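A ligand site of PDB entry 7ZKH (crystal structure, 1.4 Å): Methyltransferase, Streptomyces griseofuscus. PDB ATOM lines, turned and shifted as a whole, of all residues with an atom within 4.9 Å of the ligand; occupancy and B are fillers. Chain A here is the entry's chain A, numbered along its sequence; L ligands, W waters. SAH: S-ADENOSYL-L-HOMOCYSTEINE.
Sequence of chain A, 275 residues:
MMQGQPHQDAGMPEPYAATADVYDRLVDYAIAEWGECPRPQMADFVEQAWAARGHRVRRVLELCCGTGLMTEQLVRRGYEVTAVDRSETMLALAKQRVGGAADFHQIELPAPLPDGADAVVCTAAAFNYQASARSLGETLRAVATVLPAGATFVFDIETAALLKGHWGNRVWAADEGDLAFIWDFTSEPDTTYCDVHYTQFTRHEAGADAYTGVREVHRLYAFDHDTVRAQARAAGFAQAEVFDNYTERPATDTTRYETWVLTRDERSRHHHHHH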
ATOM      1  N   MET A   2     -28.624 -25.924  -0.450  1.00  0.00           N
ATOM      2  CA  MET A   2     -27.743 -25.706   0.707  1.00  0.00           C
ATOM      3  C   MET A   2     -28.155 -26.643   1.845  1.00  0.00           C
ATOM      4  O   MET A   2     -29.259 -26.526   2.362  1.00  0.00           O
ATOM      5  CB  MET A   2     -27.829 -24.239   1.199  1.00  0.00           C
ATOM      6  CG  MET A   2     -26.946 -23.930   2.413  1.00  0.00           C
ATOM      7  SD  MET A   2     -26.979 -22.195   2.923  1.00  0.00           S
ATOM      8  CE  MET A   2     -25.969 -22.233   4.404  1.00  0.00           C
ATOM      9  N   PRO A  15     -29.918 -18.831   1.250  1.00  0.00           N
ATOM     10  CA  PRO A  15     -29.437 -17.692   2.031  1.00  0.00           C
ATOM     11  C   PRO A  15     -28.418 -16.863   1.244  1.00  0.00           C
ATOM     12  O   PRO A  15     -27.436 -17.393   0.695  1.00  0.00           O
ATOM     13  CB  PRO A  15     -28.797 -18.335   3.260  1.00  0.00           C
ATOM     14  CG  PRO A  15     -29.643 -19.548   3.485  1.00  0.00           C
ATOM     15  CD  PRO A  15     -29.978 -20.063   2.080  1.00  0.00           C
ATOM     16  N   TYR A  16     -28.665 -15.560   1.199  1.00  0.00           N
ATOM     17  CA  TYR A  16     -27.834 -14.535   0.582  1.00  0.00           C
ATOM     18  C   TYR A  16     -27.866 -14.564  -0.931  1.00  0.00           C
ATOM     19  O   TYR A  16     -27.187 -13.729  -1.567  1.00  0.00           O
ATOM     20  CB  TYR A  16     -26.378 -14.535   1.119  1.00  0.00           C
ATOM     21  CG  TYR A  16     -26.367 -14.472   2.621  1.00  0.00           C
ATOM     22  CD1 TYR A  16     -26.635 -13.266   3.283  1.00  0.00           C
ATOM     23  CD2 TYR A  16     -26.172 -15.618   3.383  1.00  0.00           C
ATOM     24  CE1 TYR A  16     -26.667 -13.219   4.656  1.00  0.00           C
ATOM     25  CE2 TYR A  16     -26.196 -15.559   4.798  1.00  0.00           C
ATOM     26  CZ  TYR A  16     -26.434 -14.365   5.401  1.00  0.00           C
ATOM     27  OH  TYR A  16     -26.466 -14.277   6.771  1.00  0.00           O
ATOM     28  N   TYR A  23     -26.680  -6.794   2.210  1.00  0.00           N
ATOM     29  CA  TYR A  23     -26.025  -7.349   3.390  1.00  0.00           C
ATOM     30  C   TYR A  23     -25.262  -6.268   4.165  1.00  0.00           C
ATOM     31  O   TYR A  23     -25.390  -6.180   5.386  1.00  0.00           O
ATOM     32  CB  TYR A  23     -25.098  -8.511   2.996  1.00  0.00           C
ATOM     33  CG  TYR A  23     -24.368  -9.053   4.196  1.00  0.00           C
ATOM     34  CD1 TYR A  23     -24.997  -9.942   5.071  1.00  0.00           C
ATOM     35  CD2 TYR A  23     -23.031  -8.683   4.448  1.00  0.00           C
ATOM     36  CE1 TYR A  23     -24.360 -10.403   6.189  1.00  0.00           C
ATOM     37  CE2 TYR A  23     -22.369  -9.162   5.538  1.00  0.00           C
ATOM     38  CZ  TYR A  23     -23.031 -10.036   6.400  1.00  0.00           C
ATOM     39  OH  TYR A  23     -22.353 -10.480   7.515  1.00  0.00           O
ATOM     40  N   VAL A  27     -25.791  -5.179   8.001  1.00  0.00           N
ATOM     41  CA  VAL A  27     -24.729  -5.205   9.021  1.00  0.00           C
ATOM     42  C   VAL A  27     -24.640  -3.866   9.729  1.00  0.00           C
ATOM     43  O   VAL A  27     -24.506  -3.825  10.949  1.00  0.00           O
ATOM     44  CB  VAL A  27     -23.376  -5.639   8.427  1.00  0.00           C
ATOM     45  CG1 VAL A  27     -22.208  -5.330   9.407  1.00  0.00           C
ATOM     46  CG2 VAL A  27     -23.425  -7.135   8.096  1.00  0.00           C
ATOM     47  N   ARG A  39     -16.336  -4.550  12.209  1.00  0.00           N
ATOM     48  CA  ARG A  39     -15.163  -5.311  11.751  1.00  0.00           C
ATOM     49  C   ARG A  39     -13.802  -4.786  12.222  1.00  0.00           C
ATOM     50  O   ARG A  39     -12.904  -5.616  12.468  1.00  0.00           O
ATOM     51  CB  ARG A  39     -15.213  -5.594  10.247  1.00  0.00           C
ATOM     52  CG  ARG A  39     -16.498  -6.286   9.774  1.00  0.00           C
ATOM     53  CD  ARG A  39     -16.951  -7.485  10.616  1.00  0.00           C
ATOM     54  NE  ARG A  39     -18.142  -8.124  10.034  1.00  0.00           N
ATOM     55  CZ  ARG A  39     -19.396  -7.906  10.429  1.00  0.00           C
ATOM     56  NH1 ARG A  39     -19.676  -7.105  11.453  1.00  0.00           N
ATOM     57  NH2 ARG A  39     -20.394  -8.484   9.774  1.00  0.00           N
ATOM     58  N   GLU A  62      -9.640 -17.058   5.891  1.00  0.00           N
ATOM     59  CA  GLU A  62     -10.922 -16.567   6.361  1.00  0.00           C
ATOM     60  C   GLU A  62     -12.035 -17.460   5.813  1.00  0.00           C
ATOM     61  O   GLU A  62     -12.183 -17.591   4.589  1.00  0.00           O
ATOM     62  CB  GLU A  62     -11.164 -15.135   5.915  1.00  0.00           C
ATOM     63  CG  GLU A  62     -12.483 -14.645   6.463  1.00  0.00           C
ATOM     64  CD  GLU A  62     -12.897 -13.298   5.980  1.00  0.00           C
ATOM     65  OE1 GLU A  62     -12.180 -12.727   5.147  1.00  0.00           O
ATOM     66  OE2 GLU A  62     -13.964 -12.822   6.461  1.00  0.00           O
ATOM     67  N   LEU A  63     -12.825 -18.055   6.695  1.00  0.00           N
ATOM     68  CA  LEU A  63     -13.964 -18.856   6.271  1.00  0.00           C
ATOM     69  C   LEU A  63     -15.212 -17.996   6.224  1.00  0.00           C
ATOM     70  O   LEU A  63     -15.446 -17.151   7.093  1.00  0.00           O
ATOM     71  CB  LEU A  63     -14.222 -20.016   7.230  1.00  0.00           C
ATOM     72  CG  LEU A  63     -12.989 -20.792   7.635  1.00  0.00           C
ATOM     73  CD1 LEU A  63     -13.410 -21.910   8.588  1.00  0.00           C
ATOM     74  CD2 LEU A  63     -12.271 -21.342   6.396  1.00  0.00           C
ATOM     75  N   CYS A  64     -16.062 -18.287   5.255  1.00  0.00           N
ATOM     76  CA  CYS A  64     -17.379 -17.646   5.149  1.00  0.00           C
ATOM     77  C   CYS A  64     -17.236 -16.131   5.086  1.00  0.00           C
ATOM     78  O   CYS A  64     -17.857 -15.388   5.859  1.00  0.00           O
ATOM     79  CB  CYS A  64     -18.326 -18.067   6.264  1.00  0.00           C
ATOM     80  SG  CYS A  64     -18.422 -19.854   6.476  1.00  0.00           S
ATOM     81  N   CYS A  65     -16.416 -15.675   4.112  1.00  0.00           N
ATOM     82  CA  CYS A  65     -16.042 -14.277   4.051  1.00  0.00           C
ATOM     83  C   CYS A  65     -17.178 -13.354   3.646  1.00  0.00           C
ATOM     84  O   CYS A  65     -17.029 -12.117   3.789  1.00  0.00           O
ATOM     85  CB  CYS A  65     -14.884 -14.078   3.087  1.00  0.00           C
ATOM     86  SG  CYS A  65     -15.230 -14.563   1.381  1.00  0.00           S
ATOM     87  N   GLY A  66     -18.294 -13.875   3.123  1.00  0.00           N
ATOM     88  CA  GLY A  66     -19.381 -12.974   2.768  1.00  0.00           C
ATOM     89  C   GLY A  66     -18.968 -11.954   1.736  1.00  0.00           C
ATOM     90  O   GLY A  66     -18.277 -12.250   0.753  1.00  0.00           O
ATOM     91  N   THR A  67     -19.370 -10.699   1.977  1.00  0.00           N
ATOM     92  CA  THR A  67     -19.040  -9.596   1.088  1.00  0.00           C
ATOM     93  C   THR A  67     -17.649  -9.022   1.377  1.00  0.00           C
ATOM     94  O   THR A  67     -17.280  -7.959   0.835  1.00  0.00           O
ATOM     95  CB  THR A  67     -20.074  -8.476   1.226  1.00  0.00           C
ATOM     96  OG1 THR A  67     -19.976  -7.920   2.544  1.00  0.00           O
ATOM     97  CG2 THR A  67     -21.501  -8.999   0.952  1.00  0.00           C
ATOM     98  N   LEU A  69     -16.241  -7.876   4.371  1.00  0.00           N
ATOM     99  CA  LEU A  69     -16.041  -6.816   5.360  1.00  0.00           C
ATOM    100  C   LEU A  69     -14.872  -7.118   6.293  1.00  0.00           C
ATOM    101  O   LEU A  69     -14.109  -6.220   6.643  1.00  0.00           O
ATOM    102  CB  LEU A  69     -17.313  -6.585   6.172  1.00  0.00           C
ATOM    103  CG  LEU A  69     -18.473  -5.965   5.398  1.00  0.00           C
ATOM    104  CD1 LEU A  69     -19.741  -6.023   6.230  1.00  0.00           C
ATOM    105  CD2 LEU A  69     -18.158  -4.504   5.049  1.00  0.00           C
ATOM    106  N   MET A  70     -14.754  -8.360   6.752  1.00  0.00           N
ATOM    107  CA  MET A  70     -13.588  -8.713   7.562  1.00  0.00           C
ATOM    108  C   MET A  70     -12.357  -8.899   6.683  1.00  0.00           C
ATOM    109  O   MET A  70     -11.230  -8.517   7.065  1.00  0.00           O
ATOM    110  CB  MET A  70     -13.870  -9.995   8.350  1.00  0.00           C
ATOM    111  CG  MET A  70     -12.708 -10.437   9.269  1.00  0.00           C
ATOM    112  SD  MET A  70     -12.500  -9.277  10.635  1.00  0.00           S
ATOM    113  CE  MET A  70     -11.375 -10.224  11.676  1.00  0.00           C
ATOM    114  N   ASP A  85     -16.106 -18.856   0.599  1.00  0.00           N
ATOM    115  CA  ASP A  85     -17.542 -18.743   0.903  1.00  0.00           C
ATOM    116  C   ASP A  85     -18.281 -19.631  -0.067  1.00  0.00           C
ATOM    117  O   ASP A  85     -17.803 -19.893  -1.173  1.00  0.00           O
ATOM    118  CB  ASP A  85     -18.026 -17.295   0.749  1.00  0.00           C
ATOM    119  CG  ASP A  85     -19.307 -17.013   1.500  1.00  0.00           C
ATOM    120  OD1 ASP A  85     -20.409 -17.350   1.018  1.00  0.00           O
ATOM    121  OD2 ASP A  85     -19.251 -16.466   2.638  1.00  0.00           O
ATOM    122  N   ARG A  86     -19.477 -20.088   0.331  1.00  0.00           N
ATOM    123  CA  ARG A  86     -20.272 -20.913  -0.567  1.00  0.00           C
ATOM    124  C   ARG A  86     -21.043 -20.082  -1.596  1.00  0.00           C
ATOM    125  O   ARG A  86     -21.514 -20.644  -2.605  1.00  0.00           O
ATOM    126  CB  ARG A  86     -21.279 -21.765   0.234  1.00  0.00           C
ATOM    127  CG  ARG A  86     -22.369 -20.916   0.920  1.00  0.00           C
ATOM    128  CD  ARG A  86     -23.457 -21.763   1.602  1.00  0.00           C
ATOM    129  NE  ARG A  86     -24.027 -22.742   0.689  1.00  0.00           N
ATOM    130  CZ  ARG A  86     -24.950 -22.468  -0.228  1.00  0.00           C
ATOM    131  NH1 ARG A  86     -25.430 -21.235  -0.370  1.00  0.00           N
ATOM    132  NH2 ARG A  86     -25.378 -23.434  -1.028  1.00  0.00           N
ATOM    133  N   SER A  87     -21.213 -18.777  -1.376  1.00  0.00           N
ATOM    134  CA  SER A  87     -22.166 -17.943  -2.106  1.00  0.00           C
ATOM    135  C   SER A  87     -21.503 -17.157  -3.232  1.00  0.00           C
ATOM    136  O   SER A  87     -20.666 -16.299  -2.973  1.00  0.00           O
ATOM    137  CB  SER A  87     -22.829 -16.952  -1.158  1.00  0.00           C
ATOM    138  OG  SER A  87     -23.616 -16.015  -1.898  1.00  0.00           O
ATOM    139  N   MET A  90     -22.360 -13.376  -2.732  1.00  0.00           N
ATOM    140  CA  MET A  90     -21.539 -12.737  -1.706  1.00  0.00           C
ATOM    141  C   MET A  90     -20.105 -12.564  -2.196  1.00  0.00           C
ATOM    142  O   MET A  90     -19.520 -11.481  -2.030  1.00  0.00           O
ATOM    143  CB  MET A  90     -21.595 -13.569  -0.414  1.00  0.00           C
ATOM    144  CG  MET A  90     -22.978 -13.586   0.219  1.00  0.00           C
ATOM    145  SD  MET A  90     -23.597 -12.035   0.898  1.00  0.00           S
ATOM    146  CE  MET A  90     -23.029 -12.142   2.596  1.00  0.00           C
ATOM    147  N   ILE A 107     -16.279 -22.399  -1.775  1.00  0.00           N
ATOM    148  CA  ILE A 107     -16.231 -23.678  -1.074  1.00  0.00           C
ATOM    149  C   ILE A 107     -17.395 -23.714  -0.111  1.00  0.00           C
ATOM    150  O   ILE A 107     -17.632 -22.730   0.599  1.00  0.00           O
ATOM    151  CB  ILE A 107     -14.933 -23.808  -0.245  1.00  0.00           C
ATOM    152  CG1 ILE A 107     -13.691 -23.785  -1.162  1.00  0.00           C
ATOM    153  CG2 ILE A 107     -14.944 -25.084   0.580  1.00  0.00           C
ATOM    154  CD1 ILE A 107     -12.356 -23.935  -0.415  1.00  0.00           C
ATOM    155  N   GLU A 108     -18.120 -24.830  -0.084  1.00  0.00           N
ATOM    156  CA  GLU A 108     -19.161 -25.062   0.915  1.00  0.00           C
ATOM    157  C   GLU A 108     -18.615 -25.972   2.010  1.00  0.00           C
ATOM    158  O   GLU A 108     -18.253 -27.120   1.754  1.00  0.00           O
ATOM    159  CB  GLU A 108     -20.429 -25.659   0.292  1.00  0.00           C
ATOM    160  CG  GLU A 108     -21.532 -25.793   1.330  1.00  0.00           C
ATOM    161  CD  GLU A 108     -22.879 -26.196   0.734  1.00  0.00           C
ATOM    162  OE1 GLU A 108     -22.954 -27.183  -0.016  1.00  0.00           O
ATOM    163  OE2 GLU A 108     -23.881 -25.500   1.028  1.00  0.00           O
ATOM    164  N   LEU A 109     -18.534 -25.440   3.234  1.00  0.00           N
ATOM    165  CA  LEU A 109     -18.047 -26.211   4.373  1.00  0.00           C
ATOM    166  C   LEU A 109     -19.140 -27.116   4.922  1.00  0.00           C
ATOM    167  O   LEU A 109     -20.316 -26.746   4.919  1.00  0.00           O
ATOM    168  CB  LEU A 109     -17.615 -25.257   5.490  1.00  0.00           C
ATOM    169  CG  LEU A 109     -16.446 -24.359   5.082  1.00  0.00           C
ATOM    170  CD1 LEU A 109     -16.200 -23.285   6.096  1.00  0.00           C
ATOM    171  CD2 LEU A 109     -15.218 -25.231   4.904  1.00  0.00           C
ATOM    172  N   THR A 123     -16.054 -14.913  10.890  1.00  0.00           N
ATOM    173  CA  THR A 123     -16.728 -13.858  11.645  1.00  0.00           C
ATOM    174  C   THR A 123     -18.210 -13.723  11.282  1.00  0.00           C
ATOM    175  O   THR A 123     -18.658 -14.069  10.183  1.00  0.00           O
ATOM    176  CB  THR A 123     -16.015 -12.509  11.446  1.00  0.00           C
ATOM    177  OG1 THR A 123     -16.005 -12.185  10.050  1.00  0.00           O
ATOM    178  CG2 THR A 123     -14.555 -12.558  11.963  1.00  0.00           C
ATOM    179  N   ALA A 124     -18.950 -13.130  12.213  1.00  0.00           N
ATOM    180  CA  ALA A 124     -20.332 -12.693  12.009  1.00  0.00           C
ATOM    181  C   ALA A 124     -21.301 -13.867  11.871  1.00  0.00           C
ATOM    182  O   ALA A 124     -22.182 -13.871  11.020  1.00  0.00           O
ATOM    183  CB  ALA A 124     -20.480 -11.654  10.901  1.00  0.00           C
ATOM    184  N   ALA A 126     -21.356 -16.897  10.939  1.00  0.00           N
ATOM    185  CA  ALA A 126     -21.451 -17.834   9.830  1.00  0.00           C
ATOM    186  C   ALA A 126     -21.599 -19.277  10.319  1.00  0.00           C
ATOM    187  O   ALA A 126     -22.270 -20.069   9.663  1.00  0.00           O
ATOM    188  CB  ALA A 126     -20.244 -17.656   8.916  1.00  0.00           C
ATOM    189  N   TYR A 129     -24.838 -21.430  10.524  1.00  0.00           N
ATOM    190  CA  TYR A 129     -25.399 -22.157   9.377  1.00  0.00           C
ATOM    191  C   TYR A 129     -24.913 -23.589   9.307  1.00  0.00           C
ATOM    192  O   TYR A 129     -25.330 -24.315   8.404  1.00  0.00           O
ATOM    193  CB  TYR A 129     -25.100 -21.445   8.042  1.00  0.00           C
ATOM    194  CG  TYR A 129     -25.818 -20.128   7.915  1.00  0.00           C
ATOM    195  CD1 TYR A 129     -27.103 -20.053   7.352  1.00  0.00           C
ATOM    196  CD2 TYR A 129     -25.217 -18.946   8.333  1.00  0.00           C
ATOM    197  CE1 TYR A 129     -27.763 -18.832   7.229  1.00  0.00           C
ATOM    198  CE2 TYR A 129     -25.879 -17.722   8.251  1.00  0.00           C
ATOM    199  CZ  TYR A 129     -27.147 -17.666   7.672  1.00  0.00           C
ATOM    200  OH  TYR A 129     -27.801 -16.471   7.584  1.00  0.00           O
ATOM    201  N   GLN A 130     -24.059 -24.018  10.209  1.00  0.00           N
ATOM    202  CA  GLN A 130     -23.630 -25.407  10.208  1.00  0.00           C
ATOM    203  C   GLN A 130     -24.823 -26.277  10.584  1.00  0.00           C
ATOM    204  O   GLN A 130     -25.495 -26.013  11.568  1.00  0.00           O
ATOM    205  CB  GLN A 130     -22.471 -25.592  11.173  1.00  0.00           C
ATOM    206  CG  GLN A 130     -21.149 -24.991  10.655  1.00  0.00           C
ATOM    207  CD  GLN A 130     -20.648 -25.754   9.436  1.00  0.00           C
ATOM    208  OE1 GLN A 130     -20.347 -26.937   9.534  1.00  0.00           O
ATOM    209  NE2 GLN A 130     -20.575 -25.096   8.274  1.00  0.00           N
HETATM  210  N   SAH L   1     -17.833 -13.168   7.641  1.00  0.00           N
HETATM  211  CA  SAH L   1     -18.624 -12.133   6.919  1.00  0.00           C
HETATM  212  CB  SAH L   1     -19.968 -12.645   6.365  1.00  0.00           C
HETATM  213  CG  SAH L   1     -20.892 -13.303   7.372  1.00  0.00           C
HETATM  214  SD  SAH L   1     -22.539 -13.670   6.679  1.00  0.00           S
HETATM  215  C   SAH L   1     -18.777 -10.832   7.702  1.00  0.00           C
HETATM  216  O   SAH L   1     -19.591  -9.968   7.406  1.00  0.00           O
HETATM  217  OXT SAH L   1     -17.930 -10.736   8.688  1.00  0.00           O
HETATM  218  C5' SAH L   1     -22.511 -15.480   6.619  1.00  0.00           C
HETATM  219  C4' SAH L   1     -21.756 -16.007   5.409  1.00  0.00           C
HETATM  220  O4' SAH L   1     -21.542 -17.420   5.636  1.00  0.00           O
HETATM  221  C3' SAH L   1     -22.449 -15.886   4.044  1.00  0.00           C
HETATM  222  O3' SAH L   1     -21.607 -15.254   3.098  1.00  0.00           O
HETATM  223  C2' SAH L   1     -22.774 -17.341   3.695  1.00  0.00           C
HETATM  224  O2' SAH L   1     -22.847 -17.588   2.284  1.00  0.00           O
HETATM  225  C1' SAH L   1     -21.612 -18.059   4.380  1.00  0.00           C
HETATM  226  N9  SAH L   1     -21.803 -19.477   4.613  1.00  0.00           N
HETATM  227  C8  SAH L   1     -22.782 -20.044   5.398  1.00  0.00           C
HETATM  228  N7  SAH L   1     -22.673 -21.343   5.529  1.00  0.00           N
HETATM  229  C5  SAH L   1     -21.555 -21.655   4.780  1.00  0.00           C
HETATM  230  C6  SAH L   1     -20.902 -22.871   4.514  1.00  0.00           C
HETATM  231  N6  SAH L   1     -21.345 -24.064   4.953  1.00  0.00           N
HETATM  232  N1  SAH L   1     -19.785 -22.836   3.755  1.00  0.00           N
HETATM  233  C2  SAH L   1     -19.384 -21.661   3.258  1.00  0.00           C
HETATM  234  N3  SAH L   1     -19.935 -20.453   3.412  1.00  0.00           N
HETATM  235  C4  SAH L   1     -21.006 -20.518   4.210  1.00  0.00           C
HETATM  236  O   HOH W   1     -21.652 -22.446   8.208  1.00  0.00           O
HETATM  237  O   HOH W   2     -23.748 -25.120   6.170  1.00  0.00           O
HETATM  238  O   HOH W   3     -15.302 -14.471   8.082  1.00  0.00           O
HETATM  239  O   HOH W   4     -25.170 -18.907   1.463  1.00  0.00           O
HETATM  240  O   HOH W   5     -18.881  -9.373   4.674  1.00  0.00           O
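The side-chain hydroxyl of Thr 123 is in hydrogen-bond range of an oxygen (OXT) of the ligand (2.8 Å).
A nitrogen (N3) of the ligand lies within hydrogen-bond range of the backbone NH (N) of Arg 86 (3.1 Å).
The backbone carbonyl oxygen (O) of Leu 109 sits at hydrogen-bond distance from a nitrogen (N6) of the ligand (2.9 Å).
O of the ligand lies within salt-bridge range of NH2 of Arg 39.
O of Cys 64 is in hydrogen-bond range of N of the ligand (2.8 Å).
O of Thr 123 sits at hydrogen-bond distance from N of the ligand (2.8 Å).
SG of Cys 64 is in hydrogen-bond range of N3 of the ligand (3.5 Å).
OD2 of Asp 85 is in hydrogen-bond range of O3' of the ligand (2.7 Å).
N of Leu 109 is in hydrogen-bond range of N1 of the ligand (2.9 Å).
The side-chain hydroxyl (OH) of Tyr 23 lies within hydrogen-bond range of an oxygen (O) of the ligand.
The backbone NH (N) of Ser 87 is in hydrogen-bond range of the side-chain carboxylate (OD1) of Asp 85, at 2.9 Å.
OH of Tyr 129 sits at hydrogen-bond distance from OH of Tyr 16.
The side-chain hydroxyl (OG) of Ser 87 lies within hydrogen-bond range of the backbone NH (N) of Met 90 (3.0 Å).
SD of Met 2 lies close to NE of Arg 86, 3.7 Å away.
The backbone NH (N) of Cys 65 is in hydrogen-bond range of the side-chain carboxylate (OD2) of Asp 85 (3.3 Å).
The backbone NH (N) of Arg 86 is in hydrogen-bond range of the backbone carbonyl oxygen (O) of Ile 107 (3.2 Å).
The side-chain carboxylate of Asp 85 lies within hydrogen-bond range of the backbone NH of Gly 66 (2.8 Å).
The backbone carbonyl oxygen (O) of Asp 85 is in hydrogen-bond range of the backbone NH (N) of Ile 107, 3.0 Å away.
Met 2 touches the ligand (CE to N7, 3.6 Å).
Tyr 16 touches the ligand.
Cys 65 touches the ligand.
Gly 66 touches the ligand.
CB of Ser 87 touches O2' of the ligand, 3.5 Å away.
Met 90 touches the ligand (CE to O3', 3.5 Å).
O of Ile 107 touches C2 of the ligand (3.4 Å).
Glu 108 touches the ligand.
CB of Ala 124 touches OXT of the ligand, at 3.5 Å.
CB of Ala 126 touches O4' of the ligand, at 3.5 Å.
Tyr 129 touches the ligand.
Gln 130 touches the ligand.
Hydrophobic or aromatic side chains that line the ligand: Met 2, Tyr 16, Tyr 23, Met 90, Leu 109, Ala 124, Ala 126 and Tyr 129.
19 residues have an atom within 4 Å of the ligand: Met 2, Tyr 16, Tyr 23, Arg 39, Cys 64, Cys 65, Gly 66, Asp 85, Arg 86, Ser 87, Met 90, Ile 107, Glu 108, Leu 109, Thr 123, Ala 124, Ala 126, Tyr 129 and Gln 130.
The nearest printed residue that does not touch the ligand is Glu 62 (4.1 Å).
Water W4 lies within hydrogen-bond range of O2' of the ligand (2.8 Å), O of Pro 15 (2.8 Å) and NH1 of Arg 86 (3.0 Å).
Water W3 lies within hydrogen-bond range of OE2 of Glu 62 (2.7 Å), O of Leu 63 (2.9 Å), N of the ligand (2.9 Å) and N of Thr 123 (2.9 Å).
Water W5 lies within hydrogen-bond range of OG1 of Thr 67 (2.8 Å), O of the ligand (2.9 Å), N of Leu 69 (3.0 Å) and O of Cys 65 (3.4 Å).
Water W2 bridges the backbone carbonyl oxygen of Tyr 129 (2.9 Å) and a nitrogen (N6) of the ligand (2.9 Å).
Water W1 lies within hydrogen-bond range of the backbone carbonyl oxygen (O) of Ala 126, the side-chain amide nitrogen (NE2) of Gln 130 and a nitrogen (N7) of the ligand.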
